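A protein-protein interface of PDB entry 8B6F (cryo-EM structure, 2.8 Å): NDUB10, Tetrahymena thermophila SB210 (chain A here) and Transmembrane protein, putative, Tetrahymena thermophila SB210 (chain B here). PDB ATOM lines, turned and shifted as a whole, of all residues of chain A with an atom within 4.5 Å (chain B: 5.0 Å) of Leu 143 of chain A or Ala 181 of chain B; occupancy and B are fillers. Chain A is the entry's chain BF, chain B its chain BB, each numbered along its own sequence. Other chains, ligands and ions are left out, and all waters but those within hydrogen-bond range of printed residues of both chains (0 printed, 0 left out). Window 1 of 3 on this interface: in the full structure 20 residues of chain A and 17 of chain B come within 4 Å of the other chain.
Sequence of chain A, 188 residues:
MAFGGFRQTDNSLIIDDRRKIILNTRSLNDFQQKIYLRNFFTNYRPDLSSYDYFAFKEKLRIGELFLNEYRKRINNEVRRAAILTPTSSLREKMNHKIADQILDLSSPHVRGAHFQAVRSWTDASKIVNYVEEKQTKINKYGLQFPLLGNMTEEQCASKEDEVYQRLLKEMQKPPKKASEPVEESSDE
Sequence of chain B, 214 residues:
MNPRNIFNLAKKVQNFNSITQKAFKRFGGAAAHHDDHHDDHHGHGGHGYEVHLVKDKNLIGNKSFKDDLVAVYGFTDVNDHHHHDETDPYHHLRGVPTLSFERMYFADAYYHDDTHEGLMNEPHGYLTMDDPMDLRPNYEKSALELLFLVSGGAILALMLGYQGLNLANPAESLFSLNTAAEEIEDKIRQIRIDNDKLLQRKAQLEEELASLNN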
ATOM      1  N   LYS A 137       8.943  12.913  14.704  1.00  0.00           N
ATOM      2  CA  LYS A 137       8.699  13.356  13.337  1.00  0.00           C
ATOM      3  C   LYS A 137       8.896  12.213  12.350  1.00  0.00           C
ATOM      4  O   LYS A 137       8.127  12.065  11.395  1.00  0.00           O
ATOM      5  CB  LYS A 137       9.614  14.531  13.001  1.00  0.00           C
ATOM      6  CG  LYS A 137       9.209  15.289  11.750  1.00  0.00           C
ATOM      7  CD  LYS A 137      10.033  16.556  11.587  1.00  0.00           C
ATOM      8  CE  LYS A 137       9.526  17.394  10.426  1.00  0.00           C
ATOM      9  NZ  LYS A 137      10.326  18.640  10.248  1.00  0.00           N
ATOM     10  N   ILE A 138       9.926  11.393  12.564  1.00  0.00           N
ATOM     11  CA  ILE A 138      10.172  10.255  11.686  1.00  0.00           C
ATOM     12  C   ILE A 138       9.056   9.226  11.814  1.00  0.00           C
ATOM     13  O   ILE A 138       8.528   8.731  10.813  1.00  0.00           O
ATOM     14  CB  ILE A 138      11.553   9.642  11.989  1.00  0.00           C
ATOM     15  CG1 ILE A 138      12.648  10.468  11.315  1.00  0.00           C
ATOM     16  CG2 ILE A 138      11.624   8.178  11.559  1.00  0.00           C
ATOM     17  CD1 ILE A 138      14.037  10.120  11.773  1.00  0.00           C
ATOM     18  N   TYR A 141       5.550   9.310   9.888  1.00  0.00           N
ATOM     19  CA  TYR A 141       5.474   8.714   8.563  1.00  0.00           C
ATOM     20  C   TYR A 141       6.107   7.332   8.498  1.00  0.00           C
ATOM     21  O   TYR A 141       6.126   6.724   7.423  1.00  0.00           O
ATOM     22  CB  TYR A 141       6.140   9.640   7.542  1.00  0.00           C
ATOM     23  CG  TYR A 141       5.689  11.075   7.673  1.00  0.00           C
ATOM     24  CD1 TYR A 141       4.428  11.467   7.247  1.00  0.00           C
ATOM     25  CD2 TYR A 141       6.522  12.037   8.228  1.00  0.00           C
ATOM     26  CE1 TYR A 141       4.008  12.777   7.369  1.00  0.00           C
ATOM     27  CE2 TYR A 141       6.112  13.350   8.355  1.00  0.00           C
ATOM     28  CZ  TYR A 141       4.854  13.714   7.923  1.00  0.00           C
ATOM     29  OH  TYR A 141       4.440  15.019   8.045  1.00  0.00           O
ATOM     30  N   GLY A 142       6.627   6.823   9.609  1.00  0.00           N
ATOM     31  CA  GLY A 142       7.139   5.466   9.641  1.00  0.00           C
ATOM     32  C   GLY A 142       8.351   5.248   8.763  1.00  0.00           C
ATOM     33  O   GLY A 142       8.420   4.243   8.046  1.00  0.00           O
ATOM     34  N   LEU A 143       9.314   6.164   8.805  1.00  0.00           N
ATOM     35  CA  LEU A 143      10.536   6.049   8.026  1.00  0.00           C
ATOM     36  C   LEU A 143      11.599   5.213   8.722  1.00  0.00           C
ATOM     37  O   LEU A 143      12.711   5.097   8.200  1.00  0.00           O
ATOM     38  CB  LEU A 143      11.111   7.439   7.729  1.00  0.00           C
ATOM     39  CG  LEU A 143      10.275   8.391   6.876  1.00  0.00           C
ATOM     40  CD1 LEU A 143      10.531   9.826   7.284  1.00  0.00           C
ATOM     41  CD2 LEU A 143      10.596   8.186   5.408  1.00  0.00           C
ATOM     42  N   GLN A 144      11.291   4.632   9.881  1.00  0.00           N
ATOM     43  CA  GLN A 144      12.293   3.974  10.707  1.00  0.00           C
ATOM     44  C   GLN A 144      12.173   2.453  10.695  1.00  0.00           C
ATOM     45  O   GLN A 144      12.723   1.790  11.578  1.00  0.00           O
ATOM     46  CB  GLN A 144      12.210   4.502  12.141  1.00  0.00           C
ATOM     47  CG  GLN A 144      11.185   3.806  13.043  1.00  0.00           C
ATOM     48  CD  GLN A 144       9.800   3.727  12.431  1.00  0.00           C
ATOM     49  OE1 GLN A 144       9.504   4.394  11.443  1.00  0.00           O
ATOM     50  NE2 GLN A 144       8.940   2.909  13.023  1.00  0.00           N
ATOM     51  N   PHE A 145      11.478   1.876   9.711  1.00  0.00           N
ATOM     52  CA  PHE A 145      11.280   0.427   9.725  1.00  0.00           C
ATOM     53  C   PHE A 145      12.601  -0.309   9.572  1.00  0.00           C
ATOM     54  O   PHE A 145      13.006  -1.026  10.503  1.00  0.00           O
ATOM     55  CB  PHE A 145      10.284   0.010   8.644  1.00  0.00           C
ATOM     56  CG  PHE A 145      10.462  -1.411   8.184  1.00  0.00           C
ATOM     57  CD1 PHE A 145      10.450  -2.452   9.099  1.00  0.00           C
ATOM     58  CD2 PHE A 145      10.629  -1.711   6.842  1.00  0.00           C
ATOM     59  CE1 PHE A 145      10.612  -3.758   8.687  1.00  0.00           C
ATOM     60  CE2 PHE A 145      10.793  -3.017   6.424  1.00  0.00           C
ATOM     61  CZ  PHE A 145      10.785  -4.041   7.347  1.00  0.00           C
ATOM     62  N   LEU A 147      15.794   1.001   9.149  1.00  0.00           N
ATOM     63  CA  LEU A 147      16.800   1.714   9.921  1.00  0.00           C
ATOM     64  C   LEU A 147      16.154   2.314  11.160  1.00  0.00           C
ATOM     65  O   LEU A 147      15.018   2.792  11.110  1.00  0.00           O
ATOM     66  CB  LEU A 147      17.441   2.826   9.086  1.00  0.00           C
ATOM     67  CG  LEU A 147      18.441   2.437   7.994  1.00  0.00           C
ATOM     68  CD1 LEU A 147      17.846   1.471   6.987  1.00  0.00           C
ATOM     69  CD2 LEU A 147      18.942   3.683   7.287  1.00  0.00           C
ATOM     70  N   LEU B 177      16.781  10.336   7.400  1.00  0.00           N
ATOM     71  CA  LEU B 177      15.338  10.170   7.540  1.00  0.00           C
ATOM     72  C   LEU B 177      14.658  11.498   7.850  1.00  0.00           C
ATOM     73  O   LEU B 177      13.561  11.769   7.352  1.00  0.00           O
ATOM     74  CB  LEU B 177      15.029   9.137   8.622  1.00  0.00           C
ATOM     75  CG  LEU B 177      15.499   7.705   8.338  1.00  0.00           C
ATOM     76  CD1 LEU B 177      15.027   6.765   9.433  1.00  0.00           C
ATOM     77  CD2 LEU B 177      15.045   7.207   6.969  1.00  0.00           C
ATOM     78  N   ASN B 178      15.294  12.338   8.669  1.00  0.00           N
ATOM     79  CA  ASN B 178      14.727  13.651   8.952  1.00  0.00           C
ATOM     80  C   ASN B 178      14.689  14.514   7.698  1.00  0.00           C
ATOM     81  O   ASN B 178      13.716  15.243   7.470  1.00  0.00           O
ATOM     82  CB  ASN B 178      15.522  14.343  10.057  1.00  0.00           C
ATOM     83  CG  ASN B 178      15.011  15.737  10.352  1.00  0.00           C
ATOM     84  OD1 ASN B 178      15.569  16.725   9.881  1.00  0.00           O
ATOM     85  ND2 ASN B 178      13.935  15.822  11.125  1.00  0.00           N
ATOM     86  N   THR B 179      15.735  14.452   6.875  1.00  0.00           N
ATOM     87  CA  THR B 179      15.711  15.178   5.611  1.00  0.00           C
ATOM     88  C   THR B 179      14.565  14.693   4.733  1.00  0.00           C
ATOM     89  O   THR B 179      13.857  15.498   4.119  1.00  0.00           O
ATOM     90  CB  THR B 179      17.046  15.012   4.883  1.00  0.00           C
ATOM     91  OG1 THR B 179      18.121  15.371   5.759  1.00  0.00           O
ATOM     92  CG2 THR B 179      17.095  15.893   3.645  1.00  0.00           C
ATOM     93  N   ALA B 180      14.371  13.377   4.661  1.00  0.00           N
ATOM     94  CA  ALA B 180      13.270  12.830   3.877  1.00  0.00           C
ATOM     95  C   ALA B 180      11.926  13.301   4.416  1.00  0.00           C
ATOM     96  O   ALA B 180      11.022  13.637   3.643  1.00  0.00           O
ATOM     97  CB  ALA B 180      13.339  11.304   3.868  1.00  0.00           C
ATOM     98  N   ALA B 181      11.774  13.327   5.740  1.00  0.00           N
ATOM     99  CA  ALA B 181      10.519  13.780   6.332  1.00  0.00           C
ATOM    100  C   ALA B 181      10.246  15.241   6.002  1.00  0.00           C
ATOM    101  O   ALA B 181       9.109  15.614   5.694  1.00  0.00           O
ATOM    102  CB  ALA B 181      10.551  13.571   7.846  1.00  0.00           C
ATOM    103  N   GLU B 182      11.274  16.088   6.074  1.00  0.00           N
ATOM    104  CA  GLU B 182      11.094  17.493   5.732  1.00  0.00           C
ATOM    105  C   GLU B 182      10.708  17.659   4.268  1.00  0.00           C
ATOM    106  O   GLU B 182       9.850  18.484   3.936  1.00  0.00           O
ATOM    107  CB  GLU B 182      12.370  18.272   6.047  1.00  0.00           C
ATOM    108  CG  GLU B 182      12.662  18.368   7.535  1.00  0.00           C
ATOM    109  CD  GLU B 182      13.984  19.047   7.829  1.00  0.00           C
ATOM    110  OE1 GLU B 182      14.767  19.263   6.881  1.00  0.00           O
ATOM    111  OE2 GLU B 182      14.238  19.366   9.009  1.00  0.00           O
ATOM    112  N   GLU B 183      11.332  16.886   3.378  1.00  0.00           N
ATOM    113  CA  GLU B 183      10.970  16.955   1.967  1.00  0.00           C
ATOM    114  C   GLU B 183       9.529  16.515   1.749  1.00  0.00           C
ATOM    115  O   GLU B 183       8.806  17.110   0.942  1.00  0.00           O
ATOM    116  CB  GLU B 183      11.931  16.103   1.138  1.00  0.00           C
ATOM    117  CG  GLU B 183      11.847  16.374  -0.354  1.00  0.00           C
ATOM    118  CD  GLU B 183      13.070  15.884  -1.105  1.00  0.00           C
ATOM    119  OE1 GLU B 183      13.964  15.292  -0.466  1.00  0.00           O
ATOM    120  OE2 GLU B 183      13.138  16.095  -2.334  1.00  0.00           O
ATOM    121  N   ILE B 184       9.095  15.469   2.454  1.00  0.00           N
ATOM    122  CA  ILE B 184       7.706  15.031   2.356  1.00  0.00           C
ATOM    123  C   ILE B 184       6.771  16.141   2.811  1.00  0.00           C
ATOM    124  O   ILE B 184       5.732  16.392   2.188  1.00  0.00           O
ATOM    125  CB  ILE B 184       7.494  13.739   3.168  1.00  0.00           C
ATOM    126  CG1 ILE B 184       8.188  12.565   2.474  1.00  0.00           C
ATOM    127  CG2 ILE B 184       6.004  13.452   3.361  1.00  0.00           C
ATOM    128  CD1 ILE B 184       8.190  11.283   3.278  1.00  0.00           C
ATOM    129  N   GLU B 185       7.121  16.826   3.900  1.00  0.00           N
ATOM    130  CA  GLU B 185       6.284  17.919   4.382  1.00  0.00           C
ATOM    131  C   GLU B 185       6.207  19.047   3.361  1.00  0.00           C
ATOM    132  O   GLU B 185       5.137  19.626   3.148  1.00  0.00           O
ATOM    133  CB  GLU B 185       6.808  18.431   5.721  1.00  0.00           C
ATOM    134  CG  GLU B 185       6.563  17.462   6.868  1.00  0.00           C
ATOM    135  CD  GLU B 185       6.949  18.032   8.216  1.00  0.00           C
ATOM    136  OE1 GLU B 185       7.615  19.089   8.250  1.00  0.00           O
ATOM    137  OE2 GLU B 185       6.584  17.426   9.244  1.00  0.00           O
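OD1 of Asn 178 of chain B sits close to OE2 of Glu 182 of chain B. The backbone NH of Leu 143 of chain A lies within hydrogen-bond range of the backbone carbonyl oxygen of Ile 138 of chain A, at 3.4 Å.
Leu 143 of chain A touches two residues of chain B. Ala 181 of chain B touches just one residue of chain A: Leu 143 (3.8 Å). Printed residues of chain B within 4 Å of Lys 137 of chain A: Asn 178 (3.997 Å), Glu 182 (3.6 Å) and Glu 185 (3.2 Å). Printed residues of chain A within 4 Å of Asn 178 of chain B: Lys 137. Of the printed residues of chain B, Ile 138 of chain A touches Leu 177 (3.4 Å). Printed residues of chain B within 4 Å of Tyr 141 of chain A: Glu 185. The nearest residue of chain A that does not touch Ala 181 of chain B is Tyr 141 of chain A (4.3 Å).
Hydrophobic or aromatic side chains of chain A that line the printed part of chain B: Ile 138, Tyr 141 and Leu 143.
The side-chain amino group (NZ) of Lys 137 of chain A lies within salt-bridge range of the side-chain carboxylate (OE1) of Glu 185 of chain B, at 3.4 Å. The side-chain hydroxyl (OH) of Tyr 141 of chain A is in hydrogen-bond range of the side-chain carboxylate (OE2) of Glu 185 of chain B (3.4 Å).
Among the printed residues, pairs that only touch across the chains: Leu 143 of chain A with Leu 177 of chain B, Ile 138 of chain A with Leu 177 of chain B, Lys 137 of chain A with Glu 182 of chain B, Leu 143 of chain A with Ala 181 of chain B and Lys 137 of chain A with Asn 178 of chain B.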
